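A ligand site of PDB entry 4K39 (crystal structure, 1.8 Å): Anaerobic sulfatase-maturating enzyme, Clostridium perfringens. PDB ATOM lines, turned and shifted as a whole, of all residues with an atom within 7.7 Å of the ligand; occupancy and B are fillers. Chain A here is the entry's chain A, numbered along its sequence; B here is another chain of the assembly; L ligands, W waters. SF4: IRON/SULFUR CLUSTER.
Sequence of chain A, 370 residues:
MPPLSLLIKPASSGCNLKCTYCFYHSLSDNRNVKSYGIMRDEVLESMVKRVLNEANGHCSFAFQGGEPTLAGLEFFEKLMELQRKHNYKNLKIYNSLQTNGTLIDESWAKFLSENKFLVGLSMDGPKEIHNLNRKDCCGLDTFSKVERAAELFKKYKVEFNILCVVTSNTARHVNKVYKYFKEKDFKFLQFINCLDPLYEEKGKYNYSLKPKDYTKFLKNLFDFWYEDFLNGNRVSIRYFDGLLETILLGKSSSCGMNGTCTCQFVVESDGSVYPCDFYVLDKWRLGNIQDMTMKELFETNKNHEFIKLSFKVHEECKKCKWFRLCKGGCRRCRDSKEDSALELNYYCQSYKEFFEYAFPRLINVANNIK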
ATOM      1  N   SER A 254      -2.046   5.888  -9.870  1.00  0.00           N
ATOM      2  CA  SER A 254      -1.639   4.484  -9.712  1.00  0.00           C
ATOM      3  C   SER A 254      -0.130   4.330  -9.899  1.00  0.00           C
ATOM      4  O   SER A 254       0.421   4.689 -10.947  1.00  0.00           O
ATOM      5  CB  SER A 254      -2.378   3.565 -10.691  1.00  0.00           C
ATOM      6  OG  SER A 254      -3.716   3.390 -10.296  1.00  0.00           O
ATOM      7  N   CYS A 255       0.522   3.794  -8.884  1.00  0.00           N
ATOM      8  CA  CYS A 255       1.931   3.437  -8.987  1.00  0.00           C
ATOM      9  C   CYS A 255       2.088   2.369 -10.073  1.00  0.00           C
ATOM     10  O   CYS A 255       1.304   1.428 -10.128  1.00  0.00           O
ATOM     11  CB  CYS A 255       2.428   2.886  -7.651  1.00  0.00           C
ATOM     12  SG  CYS A 255       4.202   2.996  -7.519  1.00  0.00           S
ATOM     13  N   GLY A 256       3.091   2.521 -10.929  1.00  0.00           N
ATOM     14  CA  GLY A 256       3.238   1.608 -12.064  1.00  0.00           C
ATOM     15  C   GLY A 256       2.809   2.242 -13.367  1.00  0.00           C
ATOM     16  O   GLY A 256       3.145   1.759 -14.451  1.00  0.00           O
ATOM     17  N   MET A 257       2.093   3.368 -13.274  1.00  0.00           N
ATOM     18  CA  MET A 257       1.580   4.043 -14.459  1.00  0.00           C
ATOM     19  C   MET A 257       2.274   5.362 -14.736  1.00  0.00           C
ATOM     20  O   MET A 257       1.944   6.054 -15.711  1.00  0.00           O
ATOM     21  CB  MET A 257       0.065   4.229 -14.357  1.00  0.00           C
ATOM     22  CG  MET A 257      -0.706   2.885 -14.485  1.00  0.00           C
ATOM     23  SD  MET A 257      -2.484   3.138 -14.588  1.00  0.00           S
ATOM     24  CE  MET A 257      -2.628   3.701 -16.287  1.00  0.00           C
ATOM     25  N   ASN A 258       3.265   5.702 -13.913  1.00  0.00           N
ATOM     26  CA  ASN A 258       3.978   6.973 -14.070  1.00  0.00           C
ATOM     27  C   ASN A 258       5.405   6.862 -14.589  1.00  0.00           C
ATOM     28  O   ASN A 258       6.104   7.871 -14.701  1.00  0.00           O
ATOM     29  CB  ASN A 258       3.938   7.777 -12.771  1.00  0.00           C
ATOM     30  CG  ASN A 258       2.556   8.266 -12.447  1.00  0.00           C
ATOM     31  OD1 ASN A 258       1.836   8.718 -13.338  1.00  0.00           O
ATOM     32  ND2 ASN A 258       2.157   8.124 -11.203  1.00  0.00           N
ATOM     33  N   GLY A 259       5.834   5.630 -14.869  1.00  0.00           N
ATOM     34  CA  GLY A 259       7.123   5.388 -15.488  1.00  0.00           C
ATOM     35  C   GLY A 259       8.287   5.137 -14.552  1.00  0.00           C
ATOM     36  O   GLY A 259       9.306   4.581 -14.958  1.00  0.00           O
ATOM     37  N   THR A 260       8.143   5.561 -13.302  1.00  0.00           N
ATOM     38  CA  THR A 260       9.194   5.371 -12.301  1.00  0.00           C
ATOM     39  C   THR A 260       8.555   4.966 -10.970  1.00  0.00           C
ATOM     40  O   THR A 260       7.384   5.235 -10.726  1.00  0.00           O
ATOM     41  CB  THR A 260      10.039   6.649 -12.118  1.00  0.00           C
ATOM     42  OG1 THR A 260       9.214   7.682 -11.596  1.00  0.00           O
ATOM     43  CG2 THR A 260      10.646   7.115 -13.448  1.00  0.00           C
ATOM     44  N   CYS A 261       9.357   4.347 -10.126  1.00  0.00           N
ATOM     45  CA  CYS A 261       8.918   3.810  -8.829  1.00  0.00           C
ATOM     46  C   CYS A 261       8.783   4.902  -7.761  1.00  0.00           C
ATOM     47  O   CYS A 261       9.343   5.983  -7.907  1.00  0.00           O
ATOM     48  CB  CYS A 261       9.921   2.770  -8.320  1.00  0.00           C
ATOM     49  SG  CYS A 261       9.978   1.247  -9.329  1.00  0.00           S
ATOM     50  N   THR A 262       8.055   4.610  -6.700  1.00  0.00           N
ATOM     51  CA  THR A 262       7.991   5.508  -5.550  1.00  0.00           C
ATOM     52  C   THR A 262       8.153   4.654  -4.291  1.00  0.00           C
ATOM     53  O   THR A 262       7.898   3.463  -4.325  1.00  0.00           O
ATOM     54  CB  THR A 262       6.624   6.249  -5.440  1.00  0.00           C
ATOM     55  OG1 THR A 262       5.568   5.305  -5.321  1.00  0.00           O
ATOM     56  CG2 THR A 262       6.358   7.118  -6.626  1.00  0.00           C
ATOM     57  N   CYS A 263       8.592   5.247  -3.193  1.00  0.00           N
ATOM     58  CA  CYS A 263       8.711   4.445  -1.977  1.00  0.00           C
ATOM     59  C   CYS A 263       7.343   4.298  -1.318  1.00  0.00           C
ATOM     60  O   CYS A 263       6.723   5.296  -0.899  1.00  0.00           O
ATOM     61  CB  CYS A 263       9.670   5.125  -1.014  1.00  0.00           C
ATOM     62  SG  CYS A 263       9.904   4.277   0.487  1.00  0.00           S
ATOM     63  N   GLN A 264       6.873   3.045  -1.223  1.00  0.00           N
ATOM     64  CA  GLN A 264       5.535   2.764  -0.722  1.00  0.00           C
ATOM     65  C   GLN A 264       5.513   2.596   0.796  1.00  0.00           C
ATOM     66  O   GLN A 264       4.440   2.503   1.396  1.00  0.00           O
ATOM     67  CB  GLN A 264       5.000   1.503  -1.405  1.00  0.00           C
ATOM     68  CG  GLN A 264       4.778   1.664  -2.921  1.00  0.00           C
ATOM     69  CD  GLN A 264       3.689   2.675  -3.248  1.00  0.00           C
ATOM     70  OE1 GLN A 264       2.698   2.801  -2.515  1.00  0.00           O
ATOM     71  NE2 GLN A 264       3.859   3.406  -4.358  1.00  0.00           N
ATOM     72  N   PRO A 275      10.589  -0.732   0.072  1.00  0.00           N
ATOM     73  CA  PRO A 275      10.082   0.308  -0.834  1.00  0.00           C
ATOM     74  C   PRO A 275       8.824  -0.062  -1.636  1.00  0.00           C
ATOM     75  O   PRO A 275       8.160   0.832  -2.109  1.00  0.00           O
ATOM     76  CB  PRO A 275      11.265   0.568  -1.790  1.00  0.00           C
ATOM     77  CG  PRO A 275      12.054  -0.717  -1.791  1.00  0.00           C
ATOM     78  CD  PRO A 275      11.894  -1.294  -0.367  1.00  0.00           C
ATOM     79  N   CYS A 276       8.497  -1.338  -1.746  1.00  0.00           N
ATOM     80  CA  CYS A 276       7.393  -1.761  -2.617  1.00  0.00           C
ATOM     81  C   CYS A 276       6.960  -3.164  -2.181  1.00  0.00           C
ATOM     82  O   CYS A 276       7.783  -3.956  -1.745  1.00  0.00           O
ATOM     83  CB  CYS A 276       7.834  -1.768  -4.066  1.00  0.00           C
ATOM     84  SG  CYS A 276       6.609  -2.469  -5.217  1.00  0.00           S
ATOM     85  N   ASP A 277       5.663  -3.424  -2.277  1.00  0.00           N
ATOM     86  CA  ASP A 277       5.082  -4.677  -1.841  1.00  0.00           C
ATOM     87  C   ASP A 277       5.654  -5.863  -2.652  1.00  0.00           C
ATOM     88  O   ASP A 277       5.642  -7.018  -2.187  1.00  0.00           O
ATOM     89  CB  ASP A 277       3.554  -4.565  -1.999  1.00  0.00           C
ATOM     90  CG  ASP A 277       2.812  -5.657  -1.285  1.00  0.00           C
ATOM     91  OD1 ASP A 277       3.377  -6.277  -0.355  1.00  0.00           O
ATOM     92  OD2 ASP A 277       1.633  -5.882  -1.661  1.00  0.00           O
ATOM     93  N   PHE A 278       6.148  -5.587  -3.851  1.00  0.00           N
ATOM     94  CA  PHE A 278       6.741  -6.658  -4.686  1.00  0.00           C
ATOM     95  C   PHE A 278       8.159  -6.997  -4.272  1.00  0.00           C
ATOM     96  O   PHE A 278       8.734  -7.987  -4.767  1.00  0.00           O
ATOM     97  CB  PHE A 278       6.792  -6.220  -6.143  1.00  0.00           C
ATOM     98  CG  PHE A 278       5.442  -6.059  -6.774  1.00  0.00           C
ATOM     99  CD1 PHE A 278       4.459  -7.026  -6.620  1.00  0.00           C
ATOM    100  CD2 PHE A 278       5.170  -4.937  -7.565  1.00  0.00           C
ATOM    101  CE1 PHE A 278       3.204  -6.863  -7.233  1.00  0.00           C
ATOM    102  CE2 PHE A 278       3.951  -4.756  -8.146  1.00  0.00           C
ATOM    103  CZ  PHE A 278       2.961  -5.729  -8.002  1.00  0.00           C
ATOM    104  N   TYR A 279       8.723  -6.199  -3.376  1.00  0.00           N
ATOM    105  CA  TYR A 279      10.153  -6.298  -3.085  1.00  0.00           C
ATOM    106  C   TYR A 279      10.432  -6.356  -1.611  1.00  0.00           C
ATOM    107  O   TYR A 279      11.352  -5.704  -1.121  1.00  0.00           O
ATOM    108  CB  TYR A 279      10.942  -5.151  -3.737  1.00  0.00           C
ATOM    109  CG  TYR A 279      10.987  -5.240  -5.257  1.00  0.00           C
ATOM    110  CD1 TYR A 279      11.980  -5.977  -5.888  1.00  0.00           C
ATOM    111  CD2 TYR A 279      10.055  -4.594  -6.054  1.00  0.00           C
ATOM    112  CE1 TYR A 279      12.052  -6.061  -7.264  1.00  0.00           C
ATOM    113  CE2 TYR A 279      10.099  -4.691  -7.450  1.00  0.00           C
ATOM    114  CZ  TYR A 279      11.111  -5.436  -8.044  1.00  0.00           C
ATOM    115  OH  TYR A 279      11.209  -5.550  -9.431  1.00  0.00           O
ATOM    116  N   PHE A 306      16.897   1.753  -5.298  1.00  0.00           N
ATOM    117  CA  PHE A 306      15.642   1.143  -5.749  1.00  0.00           C
ATOM    118  C   PHE A 306      14.889   2.066  -6.735  1.00  0.00           C
ATOM    119  O   PHE A 306      14.520   1.649  -7.836  1.00  0.00           O
ATOM    120  CB  PHE A 306      14.753   0.775  -4.561  1.00  0.00           C
ATOM    121  CG  PHE A 306      13.467   0.107  -4.982  1.00  0.00           C
ATOM    122  CD1 PHE A 306      13.463  -1.233  -5.313  1.00  0.00           C
ATOM    123  CD2 PHE A 306      12.299   0.844  -5.132  1.00  0.00           C
ATOM    124  CE1 PHE A 306      12.298  -1.849  -5.747  1.00  0.00           C
ATOM    125  CE2 PHE A 306      11.121   0.223  -5.555  1.00  0.00           C
ATOM    126  CZ  PHE A 306      11.135  -1.123  -5.859  1.00  0.00           C
ATOM    127  N   ILE A 307      14.615   3.291  -6.355  1.00  0.00           N
ATOM    128  CA  ILE A 307      13.930   4.219  -7.224  1.00  0.00           C
ATOM    129  C   ILE A 307      14.706   4.536  -8.494  1.00  0.00           C
ATOM    130  O   ILE A 307      14.156   4.589  -9.563  1.00  0.00           O
ATOM    131  CB  ILE A 307      13.686   5.570  -6.529  1.00  0.00           C
ATOM    132  CG1 ILE A 307      12.906   5.413  -5.224  1.00  0.00           C
ATOM    133  CG2 ILE A 307      12.968   6.540  -7.433  1.00  0.00           C
ATOM    134  CD1 ILE A 307      11.959   4.271  -5.165  1.00  0.00           C
ATOM    135  N   SER A 310      14.747   2.465 -11.687  1.00  0.00           N
ATOM    136  CA  SER A 310      13.499   2.461 -12.462  1.00  0.00           C
ATOM    137  C   SER A 310      13.444   3.651 -13.422  1.00  0.00           C
ATOM    138  O   SER A 310      12.484   3.819 -14.181  1.00  0.00           O
ATOM    139  CB  SER A 310      12.293   2.524 -11.527  1.00  0.00           C
ATOM    140  OG  SER A 310      12.102   3.842 -11.017  1.00  0.00           O
ATOM    141  N   GLY A 329       5.510   1.229 -18.177  1.00  0.00           N
ATOM    142  CA  GLY A 329       4.824   0.348 -17.245  1.00  0.00           C
ATOM    143  C   GLY A 329       5.546   0.148 -15.926  1.00  0.00           C
ATOM    144  O   GLY A 329       6.553   0.807 -15.636  1.00  0.00           O
ATOM    145  N   CYS A 330       5.051  -0.790 -15.132  1.00  0.00           N
ATOM    146  CA  CYS A 330       5.570  -1.007 -13.779  1.00  0.00           C
ATOM    147  C   CYS A 330       6.945  -1.695 -13.791  1.00  0.00           C
ATOM    148  O   CYS A 330       7.162  -2.655 -14.509  1.00  0.00           O
ATOM    149  CB  CYS A 330       4.532  -1.813 -12.995  1.00  0.00           C
ATOM    150  SG  CYS A 330       5.085  -2.587 -11.487  1.00  0.00           S
ATOM    151  N   ARG A 331       7.866  -1.202 -12.968  1.00  0.00           N
ATOM    152  CA  ARG A 331       9.215  -1.782 -12.905  1.00  0.00           C
ATOM    153  C   ARG A 331       9.227  -3.292 -12.615  1.00  0.00           C
ATOM    154  O   ARG A 331      10.096  -4.024 -13.101  1.00  0.00           O
ATOM    155  CB  ARG A 331      10.068  -0.996 -11.875  1.00  0.00           C
ATOM    156  CG  ARG A 331      11.386  -1.636 -11.478  1.00  0.00           C
ATOM    157  CD  ARG A 331      11.293  -2.351 -10.134  1.00  0.00           C
ATOM    158  NE  ARG A 331      12.631  -2.566  -9.579  1.00  0.00           N
ATOM    159  CZ  ARG A 331      13.355  -1.619  -9.000  1.00  0.00           C
ATOM    160  NH1 ARG A 331      12.867  -0.378  -8.877  1.00  0.00           N
ATOM    161  NH2 ARG A 331      14.567  -1.902  -8.530  1.00  0.00           N
ATOM    162  N   ARG A 332       8.248  -3.778 -11.824  1.00  0.00           N
ATOM    163  CA  ARG A 332       8.201  -5.203 -11.470  1.00  0.00           C
ATOM    164  C   ARG A 332       8.047  -6.071 -12.728  1.00  0.00           C
ATOM    165  O   ARG A 332       8.509  -7.204 -12.775  1.00  0.00           O
ATOM    166  CB  ARG A 332       7.085  -5.449 -10.456  1.00  0.00           C
ATOM    167  CG  ARG A 332       6.776  -6.923 -10.068  1.00  0.00           C
ATOM    168  CD  ARG A 332       7.969  -7.748  -9.589  1.00  0.00           C
ATOM    169  NE  ARG A 332       7.500  -9.092  -9.195  1.00  0.00           N
ATOM    170  CZ  ARG A 332       7.309 -10.102 -10.046  1.00  0.00           C
ATOM    171  NH1 ARG A 332       6.848 -11.266  -9.624  1.00  0.00           N
ATOM    172  NH2 ARG A 332       7.567  -9.924 -11.333  1.00  0.00           N
ATOM    173  N   CYS A 333       7.416  -5.498 -13.756  1.00  0.00           N
ATOM    174  CA  CYS A 333       7.210  -6.226 -15.009  1.00  0.00           C
ATOM    175  C   CYS A 333       8.376  -6.078 -15.973  1.00  0.00           C
ATOM    176  O   CYS A 333       8.290  -6.535 -17.126  1.00  0.00           O
ATOM    177  CB  CYS A 333       5.924  -5.753 -15.677  1.00  0.00           C
ATOM    178  SG  CYS A 333       4.464  -6.363 -14.789  1.00  0.00           S
ATOM    179  N   ASP A 335      11.656  -6.468 -14.499  1.00  0.00           N
ATOM    180  CA  ASP A 335      12.750  -6.998 -13.683  1.00  0.00           C
ATOM    181  C   ASP A 335      12.812  -8.505 -13.850  1.00  0.00           C
ATOM    182  O   ASP A 335      12.286  -9.258 -13.041  1.00  0.00           O
ATOM    183  CB  ASP A 335      12.521  -6.626 -12.205  1.00  0.00           C
ATOM    184  CG  ASP A 335      13.756  -6.790 -11.349  1.00  0.00           C
ATOM    185  OD1 ASP A 335      14.874  -6.994 -11.881  1.00  0.00           O
ATOM    186  OD2 ASP A 335      13.625  -6.690 -10.107  1.00  0.00           O
ATOM    187  N   ALA B   3       0.924   8.131  -5.322  1.00  0.00           N
ATOM    188  CA  ALA B   3       0.548   6.992  -6.162  1.00  0.00           C
ATOM    189  C   ALA B   3       0.614   5.666  -5.410  1.00  0.00           C
ATOM    190  O   ALA B   3       1.650   5.343  -4.820  1.00  0.00           O
ATOM    191  CB  ALA B   3       1.410   6.931  -7.445  1.00  0.00           C
ATOM    192  N   VAL B   4      -0.478   4.897  -5.425  1.00  0.00           N
ATOM    193  CA  VAL B   4      -0.545   3.586  -4.765  1.00  0.00           C
ATOM    194  C   VAL B   4      -0.516   2.456  -5.807  1.00  0.00           C
ATOM    195  O   VAL B   4      -0.896   2.685  -6.957  1.00  0.00           O
ATOM    196  CB  VAL B   4      -1.802   3.457  -3.886  1.00  0.00           C
ATOM    197  CG1 VAL B   4      -1.503   3.922  -2.458  1.00  0.00           C
ATOM    198  CG2 VAL B   4      -2.973   4.260  -4.479  1.00  0.00           C
ATOM    199  N   PRO B   5      -0.065   1.245  -5.424  1.00  0.00           N
ATOM    200  CA  PRO B   5      -0.102   0.125  -6.380  1.00  0.00           C
ATOM    201  C   PRO B   5      -1.488  -0.535  -6.481  1.00  0.00           C
ATOM    202  O   PRO B   5      -2.304  -0.369  -5.573  1.00  0.00           O
ATOM    203  CB  PRO B   5       0.943  -0.853  -5.839  1.00  0.00           C
ATOM    204  CG  PRO B   5       0.984  -0.570  -4.351  1.00  0.00           C
ATOM    205  CD  PRO B   5       0.688   0.900  -4.203  1.00  0.00           C
ATOM    206  N   SER B   6      -1.741  -1.280  -7.574  1.00  0.00           N
ATOM    207  CA  SER B   6      -3.098  -1.735  -7.894  1.00  0.00           C
ATOM    208  C   SER B   6      -3.640  -2.824  -6.967  1.00  0.00           C
ATOM    209  O   SER B   6      -4.812  -3.199  -7.092  1.00  0.00           O
ATOM    210  CB  SER B   6      -3.218  -2.174  -9.372  1.00  0.00           C
ATOM    211  OG  SER B   6      -2.442  -3.327  -9.648  1.00  0.00           O
HETATM  212 FE1  SF4 L   1       6.442  -1.139  -7.097  1.00  0.00          FE
HETATM  213 FE2  SF4 L   1       5.334   1.059  -8.232  1.00  0.00          FE
HETATM  214 FE3  SF4 L   1       7.825   0.305  -8.842  1.00  0.00          FE
HETATM  215 FE4  SF4 L   1       5.744  -1.116  -9.778  1.00  0.00          FE
HETATM  216  S1  SF4 L   1       6.220   1.016 -10.310  1.00  0.00           S
HETATM  217  S2  SF4 L   1       7.675  -1.924  -8.866  1.00  0.00           S
HETATM  218  S3  SF4 L   1       4.325  -0.977  -7.984  1.00  0.00           S
HETATM  219  S4  SF4 L   1       7.120   0.987  -6.790  1.00  0.00           S
HETATM  220  O   HOH W   1       8.579   1.986 -12.381  1.00  0.00           O
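An iron atom (FE1) of the ligand is bound by the side-chain sulfur (SG) of Cys 276 (2.3 Å). SG of Cys 330 is bound to FE4 of the ligand (2.3 Å). The side-chain sulfur of Cys 255 binds an iron atom (FE2) of the ligand (2.4 Å). An iron atom (FE3) of the ligand is bound by the side-chain sulfur (SG) of Cys 261 (2.4 Å). A sulfur (S1) of the ligand lies close to the backbone NH of Gly 256 (3.5 Å). The backbone NH (N) of Arg 332 sits close to a sulfur (S2) of the ligand (3.5 Å). S4 of the ligand sits close to N of Thr 262 (3.7 Å).
N of Phe 278 sits close to SG of Cys 276. SG of Cys 330 sits close to N of Arg 332, at 3.4 Å. The side-chain amide nitrogen (NE2) of Gln 264 lies close to the side-chain sulfur (SG) of Cys 255 (3.2 Å). N of Cys 255 lies within hydrogen-bond range of O of Val 4 of chain B. The side-chain sulfur of Cys 261 lies close to the guanidinium group of Arg 331 (3.3 Å). The side-chain hydroxyl of Ser 310 sits at hydrogen-bond distance from the backbone NH of Cys 261, at 2.9 Å. The guanidinium group (NE) of Arg 331 sits close to the side-chain hydroxyl (OH) of Tyr 279 (3.3 Å). The guanidinium group (NH1) of Arg 331 is in hydrogen-bond range of the backbone carbonyl oxygen (O) of Phe 306.
Residues that only touch the ligand: Phe 278, Tyr 279 and Arg 331. Hydrophobic or aromatic side chains that line the ligand: Phe 278 and Tyr 279. Ten residues have an atom within 4 Å of the ligand: Cys 255, Gly 256, Cys 261, Thr 262, Cys 276, Phe 278, Tyr 279, Cys 330, Arg 331 and Arg 332. The nearest printed residue that does not touch the ligand is Pro 5 of chain B (4.01 Å).
Water W1 lies within hydrogen-bond range of S1 of the ligand, N of Arg 331 and N of Cys 261.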
